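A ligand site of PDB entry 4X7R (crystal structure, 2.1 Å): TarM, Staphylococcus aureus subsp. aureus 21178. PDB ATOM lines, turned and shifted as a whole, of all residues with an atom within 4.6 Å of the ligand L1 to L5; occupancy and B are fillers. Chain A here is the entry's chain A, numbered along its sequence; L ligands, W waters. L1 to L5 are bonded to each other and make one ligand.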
ATOM      1  N   HIS A   9      20.335 -24.224   0.873  1.00  0.00           N
ATOM      2  CA  HIS A   9      19.526 -23.917   2.034  1.00  0.00           C
ATOM      3  C   HIS A   9      19.082 -22.440   2.052  1.00  0.00           C
ATOM      4  O   HIS A   9      17.884 -22.166   2.080  1.00  0.00           O
ATOM      5  CB  HIS A   9      20.315 -24.256   3.308  1.00  0.00           C
ATOM      6  CG  HIS A   9      19.678 -23.773   4.559  1.00  0.00           C
ATOM      7  ND1 HIS A   9      18.338 -24.044   4.830  1.00  0.00           N
ATOM      8  CD2 HIS A   9      20.209 -23.082   5.595  1.00  0.00           C
ATOM      9  CE1 HIS A   9      18.098 -23.471   5.993  1.00  0.00           C
ATOM     10  NE2 HIS A   9      19.184 -22.894   6.496  1.00  0.00           N
ATOM     11  N   GLU A  10      20.050 -21.509   2.021  1.00  0.00           N
ATOM     12  CA  GLU A  10      19.824 -20.061   2.133  1.00  0.00           C
ATOM     13  C   GLU A  10      20.908 -19.283   1.453  1.00  0.00           C
ATOM     14  O   GLU A  10      21.965 -19.829   1.100  1.00  0.00           O
ATOM     15  CB  GLU A  10      19.847 -19.649   3.617  1.00  0.00           C
ATOM     16  CG  GLU A  10      21.240 -19.679   4.265  1.00  0.00           C
ATOM     17  CD  GLU A  10      21.358 -19.095   5.658  1.00  0.00           C
ATOM     18  OE1 GLU A  10      20.891 -17.962   5.888  1.00  0.00           O
ATOM     19  OE2 GLU A  10      22.007 -19.749   6.499  1.00  0.00           O
ATOM     20  N   LYS A  15      28.986 -15.189   3.727  1.00  0.00           N
ATOM     21  CA  LYS A  15      29.216 -16.610   3.420  1.00  0.00           C
ATOM     22  C   LYS A  15      30.552 -16.924   2.713  1.00  0.00           C
ATOM     23  O   LYS A  15      31.296 -16.025   2.323  1.00  0.00           O
ATOM     24  CB  LYS A  15      28.005 -17.211   2.660  1.00  0.00           C
ATOM     25  CG  LYS A  15      26.671 -17.158   3.426  1.00  0.00           C
ATOM     26  CD  LYS A  15      26.556 -18.265   4.466  1.00  0.00           C
ATOM     27  CE  LYS A  15      25.466 -18.030   5.472  1.00  0.00           C
ATOM     28  NZ  LYS A  15      25.815 -16.926   6.418  1.00  0.00           N
ATOM     29  N   GLY A  16      30.819 -18.227   2.576  1.00  0.00           N
ATOM     30  CA  GLY A  16      32.024 -18.780   1.974  1.00  0.00           C
ATOM     31  C   GLY A  16      31.883 -19.218   0.534  1.00  0.00           C
ATOM     32  O   GLY A  16      31.092 -18.667  -0.241  1.00  0.00           O
ATOM     33  N   GLY A  17      32.672 -20.229   0.183  1.00  0.00           N
ATOM     34  CA  GLY A  17      32.855 -20.695  -1.188  1.00  0.00           C
ATOM     35  C   GLY A  17      31.680 -21.296  -1.903  1.00  0.00           C
ATOM     36  O   GLY A  17      31.595 -21.138  -3.123  1.00  0.00           O
ATOM     37  N   MET A  18      30.803 -22.014  -1.210  1.00  0.00           N
ATOM     38  CA  MET A  18      29.680 -22.653  -1.912  1.00  0.00           C
ATOM     39  C   MET A  18      28.768 -21.662  -2.567  1.00  0.00           C
ATOM     40  O   MET A  18      28.454 -21.833  -3.738  1.00  0.00           O
ATOM     41  CB  MET A  18      28.896 -23.642  -1.007  1.00  0.00           C
ATOM     42  CG  MET A  18      27.551 -24.124  -1.618  1.00  0.00           C
ATOM     43  SD  MET A  18      26.730 -25.449  -0.715  1.00  0.00           S
ATOM     44  CE  MET A  18      26.259 -24.561   0.808  1.00  0.00           C
ATOM     45  N   THR A  19      28.349 -20.593  -1.843  1.00  0.00           N
ATOM     46  CA  THR A  19      27.459 -19.592  -2.459  1.00  0.00           C
ATOM     47  C   THR A  19      28.214 -18.717  -3.405  1.00  0.00           C
ATOM     48  O   THR A  19      27.684 -18.355  -4.449  1.00  0.00           O
ATOM     49  CB  THR A  19      26.562 -18.860  -1.447  1.00  0.00           C
ATOM     50  OG1 THR A  19      27.391 -18.233  -0.476  1.00  0.00           O
ATOM     51  CG2 THR A  19      25.558 -19.783  -0.769  1.00  0.00           C
ATOM     52  N   PHE A  41      15.361 -22.380   0.685  1.00  0.00           N
ATOM     53  CA  PHE A  41      14.289 -23.006   1.441  1.00  0.00           C
ATOM     54  C   PHE A  41      14.134 -22.486   2.865  1.00  0.00           C
ATOM     55  O   PHE A  41      13.193 -22.870   3.533  1.00  0.00           O
ATOM     56  CB  PHE A  41      14.453 -24.558   1.416  1.00  0.00           C
ATOM     57  CG  PHE A  41      14.580 -25.124   0.013  1.00  0.00           C
ATOM     58  CD1 PHE A  41      13.441 -25.332  -0.770  1.00  0.00           C
ATOM     59  CD2 PHE A  41      15.823 -25.438  -0.527  1.00  0.00           C
ATOM     60  CE1 PHE A  41      13.555 -25.839  -2.079  1.00  0.00           C
ATOM     61  CE2 PHE A  41      15.947 -25.924  -1.828  1.00  0.00           C
ATOM     62  CZ  PHE A  41      14.804 -26.109  -2.604  1.00  0.00           C
ATOM     63  N   ASP A  42      14.993 -21.579   3.319  1.00  0.00           N
ATOM     64  CA  ASP A  42      14.867 -21.053   4.671  1.00  0.00           C
ATOM     65  C   ASP A  42      13.846 -19.907   4.736  1.00  0.00           C
ATOM     66  O   ASP A  42      13.442 -19.341   3.706  1.00  0.00           O
ATOM     67  CB  ASP A  42      16.238 -20.535   5.167  1.00  0.00           C
ATOM     68  CG  ASP A  42      16.696 -19.316   4.396  1.00  0.00           C
ATOM     69  OD1 ASP A  42      16.560 -19.325   3.151  1.00  0.00           O
ATOM     70  OD2 ASP A  42      17.215 -18.379   5.029  1.00  0.00           O
ATOM     71  N   ASN A 185      13.045 -32.004  18.834  1.00  0.00           N
ATOM     72  CA  ASN A 185      14.147 -31.865  17.876  1.00  0.00           C
ATOM     73  C   ASN A 185      14.064 -30.639  16.963  1.00  0.00           C
ATOM     74  O   ASN A 185      14.934 -30.476  16.083  1.00  0.00           O
ATOM     75  CB  ASN A 185      14.310 -33.151  17.043  1.00  0.00           C
ATOM     76  CG  ASN A 185      13.113 -33.536  16.197  1.00  0.00           C
ATOM     77  OD1 ASN A 185      12.202 -32.748  15.942  1.00  0.00           O
ATOM     78  ND2 ASN A 185      13.090 -34.767  15.734  1.00  0.00           N
ATOM     79  N   GLY A 186      13.012 -29.836  17.104  1.00  0.00           N
ATOM     80  CA  GLY A 186      12.782 -28.639  16.283  1.00  0.00           C
ATOM     81  C   GLY A 186      12.418 -28.931  14.843  1.00  0.00           C
ATOM     82  O   GLY A 186      12.437 -28.013  14.014  1.00  0.00           O
ATOM     83  N   ALA A 187      12.056 -30.189  14.507  1.00  0.00           N
ATOM     84  CA  ALA A 187      11.689 -30.555  13.135  1.00  0.00           C
ATOM     85  C   ALA A 187      10.261 -30.069  12.825  1.00  0.00           C
ATOM     86  O   ALA A 187       9.402 -30.041  13.708  1.00  0.00           O
ATOM     87  CB  ALA A 187      11.759 -32.054  12.942  1.00  0.00           C
ATOM     88  N   ASN A 202       5.235 -32.588   6.146  1.00  0.00           N
ATOM     89  CA  ASN A 202       6.453 -31.990   6.712  1.00  0.00           C
ATOM     90  C   ASN A 202       7.047 -30.981   5.720  1.00  0.00           C
ATOM     91  O   ASN A 202       6.481 -30.788   4.652  1.00  0.00           O
ATOM     92  CB  ASN A 202       7.481 -33.083   7.150  1.00  0.00           C
ATOM     93  CG  ASN A 202       7.832 -34.067   6.044  1.00  0.00           C
ATOM     94  OD1 ASN A 202       7.696 -33.800   4.850  1.00  0.00           O
ATOM     95  ND2 ASN A 202       8.226 -35.263   6.418  1.00  0.00           N
ATOM     96  N   ASN A 203       8.139 -30.310   6.092  1.00  0.00           N
ATOM     97  CA  ASN A 203       8.818 -29.306   5.258  1.00  0.00           C
ATOM     98  C   ASN A 203       9.354 -29.854   3.935  1.00  0.00           C
ATOM     99  O   ASN A 203       9.280 -29.160   2.913  1.00  0.00           O
ATOM    100  CB  ASN A 203       9.944 -28.640   6.055  1.00  0.00           C
ATOM    101  CG  ASN A 203      10.480 -27.422   5.387  1.00  0.00           C
ATOM    102  OD1 ASN A 203       9.749 -26.457   5.127  1.00  0.00           O
ATOM    103  ND2 ASN A 203      11.729 -27.470   5.000  1.00  0.00           N
ATOM    104  N   LEU A 204       9.880 -31.084   3.924  1.00  0.00           N
ATOM    105  CA  LEU A 204      10.407 -31.703   2.699  1.00  0.00           C
ATOM    106  C   LEU A 204       9.276 -31.847   1.702  1.00  0.00           C
ATOM    107  O   LEU A 204       9.449 -31.452   0.568  1.00  0.00           O
ATOM    108  CB  LEU A 204      11.080 -33.060   3.040  1.00  0.00           C
ATOM    109  CG  LEU A 204      11.422 -34.008   1.897  1.00  0.00           C
ATOM    110  CD1 LEU A 204      12.532 -33.419   0.989  1.00  0.00           C
ATOM    111  CD2 LEU A 204      11.851 -35.371   2.464  1.00  0.00           C
ATOM    112  N   GLY A 229      22.491 -31.106   2.039  1.00  0.00           N
ATOM    113  CA  GLY A 229      21.333 -31.453   2.852  1.00  0.00           C
ATOM    114  C   GLY A 229      20.025 -31.203   2.104  1.00  0.00           C
ATOM    115  O   GLY A 229      18.984 -31.756   2.479  1.00  0.00           O
ATOM    116  N   SER A 230      20.090 -30.377   1.015  1.00  0.00           N
ATOM    117  CA  SER A 230      18.923 -30.085   0.173  1.00  0.00           C
ATOM    118  C   SER A 230      18.655 -31.117  -0.902  1.00  0.00           C
ATOM    119  O   SER A 230      17.617 -31.045  -1.550  1.00  0.00           O
ATOM    120  CB  SER A 230      19.059 -28.707  -0.476  1.00  0.00           C
ATOM    121  OG  SER A 230      18.603 -27.759   0.474  1.00  0.00           O
ATOM    122  N   LYS A 233      15.107 -32.759  -1.473  1.00  0.00           N
ATOM    123  CA  LYS A 233      14.065 -31.883  -2.073  1.00  0.00           C
ATOM    124  C   LYS A 233      14.025 -32.039  -3.566  1.00  0.00           C
ATOM    125  O   LYS A 233      12.933 -32.214  -4.122  1.00  0.00           O
ATOM    126  CB  LYS A 233      14.248 -30.410  -1.681  1.00  0.00           C
ATOM    127  CG  LYS A 233      14.158 -30.215  -0.180  1.00  0.00           C
ATOM    128  CD  LYS A 233      14.639 -28.863   0.217  1.00  0.00           C
ATOM    129  CE  LYS A 233      14.342 -28.617   1.671  1.00  0.00           C
ATOM    130  NZ  LYS A 233      15.522 -28.917   2.521  1.00  0.00           N
ATOM    131  N   ARG A 326      36.171 -18.780   5.834  1.00  0.00           N
ATOM    132  CA  ARG A 326      35.156 -18.959   6.875  1.00  0.00           C
ATOM    133  C   ARG A 326      36.026 -19.447   8.048  1.00  0.00           C
ATOM    134  O   ARG A 326      36.925 -20.278   7.822  1.00  0.00           O
ATOM    135  CB  ARG A 326      34.177 -20.080   6.509  1.00  0.00           C
ATOM    136  CG  ARG A 326      33.191 -19.776   5.411  1.00  0.00           C
ATOM    137  CD  ARG A 326      32.248 -20.950   5.179  1.00  0.00           C
ATOM    138  NE  ARG A 326      32.951 -22.135   4.682  1.00  0.00           N
ATOM    139  CZ  ARG A 326      32.896 -23.333   5.234  1.00  0.00           C
ATOM    140  NH1 ARG A 326      32.147 -23.550   6.299  1.00  0.00           N
ATOM    141  NH2 ARG A 326      33.585 -24.349   4.715  1.00  0.00           N
ATOM    142  N   VAL A 328      36.329 -21.728  10.418  1.00  0.00           N
ATOM    143  CA  VAL A 328      35.763 -23.017  10.824  1.00  0.00           C
ATOM    144  C   VAL A 328      36.847 -24.063  11.133  1.00  0.00           C
ATOM    145  O   VAL A 328      37.956 -23.929  10.623  1.00  0.00           O
ATOM    146  CB  VAL A 328      34.691 -23.543   9.821  1.00  0.00           C
ATOM    147  CG1 VAL A 328      33.442 -22.671   9.823  1.00  0.00           C
ATOM    148  CG2 VAL A 328      35.246 -23.727   8.400  1.00  0.00           C
HETATM  149  C1  LIG L   1      14.506 -36.134  11.850  1.00  0.00           C
HETATM  150  C2  LIG L   1      12.274 -36.848  12.329  1.00  0.00           C
HETATM  151  C3  LIG L   1      15.638 -35.203  12.346  1.00  0.00           C
HETATM  152  C4  LIG L   1      15.490 -33.813  11.743  1.00  0.00           C
HETATM  153  C5  LIG L   1      15.327 -33.811  10.203  1.00  0.00           C
HETATM  154  C6  LIG L   1      14.238 -34.851   9.776  1.00  0.00           C
HETATM  155  C7  LIG L   1      14.178 -35.046   8.243  1.00  0.00           C
HETATM  156  O1  LIG L   1      13.231 -35.790  12.455  1.00  0.00           O
HETATM  157  N1  LIG L   1      15.685 -35.107  13.798  1.00  0.00           N
HETATM  158  S1  LIG L   1      16.813 -36.252  14.514  1.00  0.00           S
HETATM  159  O2  LIG L   1      16.504 -37.652  13.970  1.00  0.00           O
HETATM  160  O3  LIG L   1      16.627 -36.141  16.035  1.00  0.00           O
HETATM  161  O4  LIG L   1      18.246 -35.867  14.140  1.00  0.00           O
HETATM  162  O5  LIG L   1      16.603 -33.029  12.168  1.00  0.00           O
HETATM  163  O6  LIG L   1      14.915 -32.479   9.843  1.00  0.00           O
HETATM  164  O7  LIG L   1      14.497 -36.152  10.393  1.00  0.00           O
HETATM  165  O8  LIG L   1      13.283 -36.125   7.914  1.00  0.00           O
HETATM  166  S2  LIG L   1      11.766 -35.947   7.704  1.00  0.00           S
HETATM  167  O9  LIG L   1      11.090 -37.318   7.841  1.00  0.00           O
HETATM  168  O10 LIG L   1      11.516 -35.411   6.293  1.00  0.00           O
HETATM  169  O11 LIG L   1      11.155 -34.985   8.744  1.00  0.00           O
HETATM  170  C1  LG2 L   2      15.580 -31.862   8.728  1.00  0.00           C
HETATM  171  C2  LG2 L   2      14.804 -30.581   8.346  1.00  0.00           C
HETATM  172  C3  LG2 L   2      15.196 -29.361   9.267  1.00  0.00           C
HETATM  173  C4  LG2 L   2      16.709 -29.241   9.493  1.00  0.00           C
HETATM  174  C5  LG2 L   2      17.310 -30.606   9.914  1.00  0.00           C
HETATM  175  C6  LG2 L   2      18.837 -30.535  10.096  1.00  0.00           C
HETATM  176  O1  LG2 L   2      15.016 -30.276   6.941  1.00  0.00           O
HETATM  177  O2  LG2 L   2      14.552 -29.429  10.552  1.00  0.00           O
HETATM  178  O3  LG2 L   2      17.334 -28.824   8.284  1.00  0.00           O
HETATM  179  O4  LG2 L   2      16.999 -31.578   8.876  1.00  0.00           O
HETATM  180  O5  LG2 L   2      19.527 -31.219   9.310  1.00  0.00           O
HETATM  181  O6  LG2 L   2      19.275 -29.790  11.006  1.00  0.00           O
HETATM  182  S1  LG2 L   2      14.062 -30.763   5.838  1.00  0.00           S
HETATM  183  O7  LG2 L   2      13.672 -32.237   5.983  1.00  0.00           O
HETATM  184  O8  LG2 L   2      12.812 -29.897   5.889  1.00  0.00           O
HETATM  185  O9  LG2 L   2      14.745 -30.614   4.482  1.00  0.00           O
HETATM  186  N1  LG3 L   3      16.718 -27.697   5.802  1.00  0.00           N
HETATM  187  C1  LG3 L   3      17.349 -27.380   8.161  1.00  0.00           C
HETATM  188  S1  LG3 L   3      15.532 -26.508   5.285  1.00  0.00           S
HETATM  189  C2  LG3 L   3      17.684 -27.062   6.715  1.00  0.00           C
HETATM  190  S2  LG3 L   3      21.325 -24.073  10.223  1.00  0.00           S
HETATM  191  C3  LG3 L   3      19.139 -27.500   6.402  1.00  0.00           C
HETATM  192  O1  LG3 L   3      19.505 -27.101   5.062  1.00  0.00           O
HETATM  193  S3  LG3 L   3      19.765 -28.182   4.019  1.00  0.00           S
HETATM  194  C4  LG3 L   3      20.157 -26.949   7.407  1.00  0.00           C
HETATM  195  O2  LG3 L   3      21.360 -27.629   7.125  1.00  0.00           O
HETATM  196  C5  LG3 L   3      19.677 -27.240   8.875  1.00  0.00           C
HETATM  197  O3  LG3 L   3      18.307 -26.746   9.045  1.00  0.00           O
HETATM  198  C6  LG3 L   3      20.471 -26.499   9.948  1.00  0.00           C
HETATM  199  O4  LG3 L   3      20.365 -25.106   9.668  1.00  0.00           O
HETATM  200  O5  LG3 L   3      16.224 -25.458   4.411  1.00  0.00           O
HETATM  201  O6  LG3 L   3      14.464 -27.268   4.517  1.00  0.00           O
HETATM  202  O7  LG3 L   3      14.916 -25.805   6.495  1.00  0.00           O
HETATM  203  O8  LG3 L   3      21.062 -22.746   9.506  1.00  0.00           O
HETATM  204  O9  LG3 L   3      21.076 -23.953  11.731  1.00  0.00           O
HETATM  205  O10 LG3 L   3      22.773 -24.512   9.963  1.00  0.00           O
HETATM  206  O11 LG3 L   3      20.861 -29.082   4.575  1.00  0.00           O
HETATM  207  O12 LG3 L   3      20.243 -27.583   2.701  1.00  0.00           O
HETATM  208  O13 LG3 L   3      18.504 -29.008   3.783  1.00  0.00           O
HETATM  209  C1  LG4 L   4      22.468 -26.722   7.225  1.00  0.00           C
HETATM  210  C2  LG4 L   4      23.673 -27.497   7.829  1.00  0.00           C
HETATM  211  C3  LG4 L   4      24.921 -26.608   7.847  1.00  0.00           C
HETATM  212  C4  LG4 L   4      25.143 -25.890   6.458  1.00  0.00           C
HETATM  213  C5  LG4 L   4      23.820 -25.208   5.999  1.00  0.00           C
HETATM  214  C6  LG4 L   4      23.947 -24.504   4.627  1.00  0.00           C
HETATM  215  O1  LG4 L   4      23.356 -27.900   9.157  1.00  0.00           O
HETATM  216  O2  LG4 L   4      26.065 -27.410   8.198  1.00  0.00           O
HETATM  217  O3  LG4 L   4      26.124 -24.863   6.654  1.00  0.00           O
HETATM  218  O4  LG4 L   4      22.757 -26.201   5.922  1.00  0.00           O
HETATM  219  O5  LG4 L   4      24.038 -25.238   3.613  1.00  0.00           O
HETATM  220  O6  LG4 L   4      23.866 -23.252   4.617  1.00  0.00           O
HETATM  221  C1  LG5 L   5      27.358 -25.135   5.947  1.00  0.00           C
HETATM  222  C2  LG5 L   5      28.546 -24.660   6.834  1.00  0.00           C
HETATM  223  C3  LG5 L   5      28.561 -23.105   7.007  1.00  0.00           C
HETATM  224  C4  LG5 L   5      28.378 -22.370   5.666  1.00  0.00           C
HETATM  225  C5  LG5 L   5      27.204 -22.968   4.845  1.00  0.00           C
HETATM  226  C6  LG5 L   5      27.064 -22.289   3.485  1.00  0.00           C
HETATM  227  N1  LG5 L   5      28.514 -25.337   8.133  1.00  0.00           N
HETATM  228  O1  LG5 L   5      29.806 -22.678   7.596  1.00  0.00           O
HETATM  229  O2  LG5 L   5      28.146 -20.967   5.888  1.00  0.00           O
HETATM  230  O3  LG5 L   5      27.351 -24.421   4.677  1.00  0.00           O
HETATM  231  O4  LG5 L   5      28.296 -22.468   2.783  1.00  0.00           O
HETATM  232  S1  LG5 L   5      29.708 -26.587   8.239  1.00  0.00           S
HETATM  233  O5  LG5 L   5      31.100 -25.965   8.177  1.00  0.00           O
HETATM  234  O6  LG5 L   5      29.543 -27.591   7.079  1.00  0.00           O
HETATM  235  O7  LG5 L   5      29.493 -27.305   9.574  1.00  0.00           O
HETATM  236  S2  LG5 L   5      29.087 -21.262   2.299  1.00  0.00           S
HETATM  237  O8  LG5 L   5      30.445 -21.788   1.824  1.00  0.00           O
HETATM  238  O9  LG5 L   5      29.300 -20.213   3.383  1.00  0.00           O
HETATM  239  O10 LG5 L   5      28.288 -20.662   1.143  1.00  0.00           O
HETATM  240  O1  LG6 L   6      29.612 -27.405   3.298  1.00  0.00           O
HETATM  241  C1  LG6 L   6      31.196 -25.145   0.765  1.00  0.00           C
HETATM  242  C2  LG6 L   6      31.019 -25.902   2.055  1.00  0.00           C
HETATM  243  O2  LG6 L   6      32.785 -25.276  -1.865  1.00  0.00           O
HETATM  244  C3  LG6 L   6      29.787 -26.776   2.040  1.00  0.00           C
HETATM  245  C4  LG6 L   6      33.774 -24.468  -2.503  1.00  0.00           C
HETATM  246  C5  LG6 L   6      33.189 -24.036  -3.831  1.00  0.00           C
HETATM  247  C6  LG6 L   6      35.075 -25.267  -2.609  1.00  0.00           C
HETATM  248  O3  LG6 L   6      32.853 -25.148  -4.645  1.00  0.00           O
HETATM  249  C7  LG6 L   6      35.599 -25.514  -1.199  1.00  0.00           C
HETATM  250  O4  LG6 L   6      36.048 -24.531  -3.343  1.00  0.00           O
HETATM  251  O5  LG6 L   6      36.805 -26.274  -1.212  1.00  0.00           O
HETATM  252  O6  LG6 L   6      35.350 -28.204   1.410  1.00  0.00           O
HETATM  253  C8  LG6 L   6      35.348 -27.053   1.836  1.00  0.00           C
HETATM  254  C9  LG6 L   6      35.840 -26.714   3.199  1.00  0.00           C
HETATM  255  N1  LG6 L   6      34.918 -26.029   1.091  1.00  0.00           N
HETATM  256  C10 LG6 L   6      34.539 -26.155  -0.305  1.00  0.00           C
HETATM  257  C11 LG6 L   6      33.095 -25.684  -0.535  1.00  0.00           C
HETATM  258  O7  LG6 L   6      32.561 -24.848   0.452  1.00  0.00           O
HETATM  259  O8  LG6 L   6      30.932 -24.967   3.134  1.00  0.00           O
HETATM  260  N1  LG7 L   7      35.294 -14.987   1.550  1.00  0.00           N
HETATM  261  C1  LG7 L   7      35.115 -13.612   1.464  1.00  0.00           C
HETATM  262  N2  LG7 L   7      35.448 -12.909   2.598  1.00  0.00           N
HETATM  263  C2  LG7 L   7      35.901 -13.422   3.792  1.00  0.00           C
HETATM  264  C3  LG7 L   7      36.015 -14.858   3.828  1.00  0.00           C
HETATM  265  C4  LG7 L   7      35.723 -15.584   2.733  1.00  0.00           C
HETATM  266  O1  LG7 L   7      34.703 -13.060   0.461  1.00  0.00           O
HETATM  267  O2  LG7 L   7      36.194 -12.643   4.717  1.00  0.00           O
HETATM  268  C5  LG7 L   7      35.140 -15.749   0.289  1.00  0.00           C
HETATM  269  C6  LG7 L   7      36.442 -15.943  -0.489  1.00  0.00           C
HETATM  270  O3  LG7 L   7      36.700 -14.830  -1.328  1.00  0.00           O
HETATM  271  C7  LG7 L   7      36.129 -17.207  -1.291  1.00  0.00           C
HETATM  272  C8  LG7 L   7      35.228 -17.997  -0.353  1.00  0.00           C
HETATM  273  O4  LG7 L   7      34.680 -17.049   0.600  1.00  0.00           O
HETATM  274  O5  LG7 L   7      35.543 -17.003  -2.584  1.00  0.00           O
HETATM  275  C9  LG7 L   7      35.893 -19.136   0.368  1.00  0.00           C
HETATM  276  O6  LG7 L   7      36.094 -20.183  -0.609  1.00  0.00           O
HETATM  277  P1  LG7 L   7      36.872 -21.559  -0.355  1.00  0.00           P
HETATM  278  O7  LG7 L   7      36.581 -22.489  -1.461  1.00  0.00           O
HETATM  279  O8  LG7 L   7      38.372 -21.260  -0.266  1.00  0.00           O
HETATM  280  O9  LG7 L   7      36.380 -22.156   1.004  1.00  0.00           O
HETATM  281  P2  LG7 L   7      34.919 -22.480   1.596  1.00  0.00           P
HETATM  282  O10 LG7 L   7      34.016 -22.961   0.491  1.00  0.00           O
HETATM  283  O11 LG7 L   7      34.319 -21.216   2.233  1.00  0.00           O
HETATM  284  O12 LG7 L   7      35.040 -23.580   2.630  1.00  0.00           O
HETATM  285  O   HOH W   1      16.454 -31.753   2.437  1.00  0.00           O
HETATM  286  O   HOH W   2      22.044 -30.114   9.051  1.00  0.00           O
HETATM  287  O   HOH W   3      12.088 -29.632   9.696  1.00  0.00           O
HETATM  288  O   HOH W   4      15.498 -30.924  13.389  1.00  0.00           O
HETATM  289  O   HOH W   5      18.762 -32.569   7.317  1.00  0.00           O
HETATM  290  O   HOH W   6      12.868 -26.524   8.526  1.00  0.00           O
HETATM  291  O   HOH W   7      15.174 -33.757   4.161  1.00  0.00           O
HETATM  292  O   HOH W   8      17.305 -26.924   2.548  1.00  0.00           O
HETATM  293  O   HOH W   9      23.289 -28.725   3.226  1.00  0.00           O
HETATM  294  O   HOH W  10      23.618 -21.909   6.672  1.00  0.00           O
HETATM  295  O   HOH W  11      17.844 -31.022   5.341  1.00  0.00           O
HETATM  296  O   HOH W  12      24.013 -21.464   2.541  1.00  0.00           O
HETATM  297  O   HOH W  13      21.757 -30.910   6.520  1.00  0.00           O
HETATM  298  O   HOH W  14      11.172 -32.765   6.602  1.00  0.00           O
HETATM  299  O   HOH W  15      22.327 -26.406   1.990  1.00  0.00           O
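N of Met 18 sits at hydrogen-bond distance from O8 of LG5 L5 (3.1 Å). ND2 of Asn 202 is in hydrogen-bond range of O10 of LIG L1, at 3.3 Å. The backbone NH of Gly 17 is in hydrogen-bond range of an oxygen (O8) of LG5 L5 (3.2 Å). An oxygen (O12) of LG3 L3 lies within hydrogen-bond range of the backbone NH (N) of Ser 230, 3.3 Å away. An oxygen (O9) of LG2 L2 is in salt-bridge range of the side-chain amino group (NZ) of Lys 233 (2.7 Å). An oxygen (O13) of LG3 L3 sits close to the backbone carbonyl oxygen (O) of Gly 229 (3.1 Å). O6 of LG3 L3 sits at hydrogen-bond distance from ND2 of Asn 203 (2.8 Å). The guanidinium group (NH2) of Arg 326 is in hydrogen-bond range of an oxygen (O8) of LG6 L6 (3.1 Å). The side-chain amide nitrogen (ND2) of Asn 185 lies close to a nitrogen (N1) of LIG L1 (3.3 Å). The backbone NH (N) of Gly 17 lies within hydrogen-bond range of an oxygen (O11) of LG7 L7. NH2 of Arg 326 lies within salt-bridge range of O12 of LG7 L7, 2.7 Å away. The backbone NH (N) of Gly 16 sits at hydrogen-bond distance from an oxygen (O9) of LG5 L5, at 2.6 Å. O10 of LG5 L5 lies within hydrogen-bond range of OG1 of Thr 19 (3.1 Å). An oxygen (O12) of LG3 L3 lies within hydrogen-bond range of the side-chain hydroxyl of Ser 230. The guanidinium group (NH1) of Arg 326 lies within salt-bridge range of an oxygen (O5) of LG5 L5, at 3.2 Å. A ring nitrogen (ND1) of His 9 sits at hydrogen-bond distance from an oxygen (O5) of LG3 L3. An oxygen (O10) of LG5 L5 is in hydrogen-bond range of the backbone NH (N) of Thr 19.
CB of Lys 15 touches O9 of LG5 L5 (3.3 Å). Phe 41 touches the ligand L1 to L5. N of Leu 204 touches O8 of LG2 L2 (3.7 Å). Hydrophobic or aromatic side chains that line the ligand L1 to L5: His 9, Met 18, Phe 41 and Leu 204. Within 4 Å of the ligand L1 to L5: His 9, Lys 15, Gly 16, Gly 17, Met 18, Thr 19, Phe 41, Asn 185, Asn 202, Asn 203, Leu 204, Gly 229, Ser 230, Lys 233 and Arg 326. The nearest printed residue that does not touch the ligand L1 to L5 is Ala 187 (4.02 Å).
An oxygen (O8) of LG6 L6 is in hydrogen-bond range of an oxygen (O8) of LG5 L5 (3.5 Å). An oxygen (O7) of LG7 L7 lies within hydrogen-bond range of an oxygen (O4) of LG6 L6, at 2.8 Å.
Water W15 bridges O12 of LG3 L3 (2.5 Å) and N of His 9 (3.2 Å). Water W8 lies within hydrogen-bond range of OG of Ser 230 (2.6 Å), O5 of LG3 L3 (2.6 Å) and NZ of Lys 233 (2.7 Å). Water W14 bridges an oxygen (O7) of LG2 L2 (2.6 Å) and the backbone NH of Leu 204 (3.4 Å). Water W11 bridges an oxygen (O13) of LG3 L3 (2.6 Å) and the backbone carbonyl oxygen of Gly 229 (3.2 Å). Water W4 bridges O5 of LIG L1 (2.7 Å) and O of Asn 185 (2.8 Å). Water W12 bridges an oxygen (O6) of LG4 L4 (2.7 Å) and the backbone carbonyl oxygen (O) of Glu 10 (3.0 Å).
N of Asp 42 sits at hydrogen-bond distance from O of His 9, 3.2 Å away. The backbone NH (N) of Ala 187 sits at hydrogen-bond distance from the side-chain amide oxygen (OD1) of Asn 185. N of Phe 41 is in hydrogen-bond range of O of His 9 (2.9 Å).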
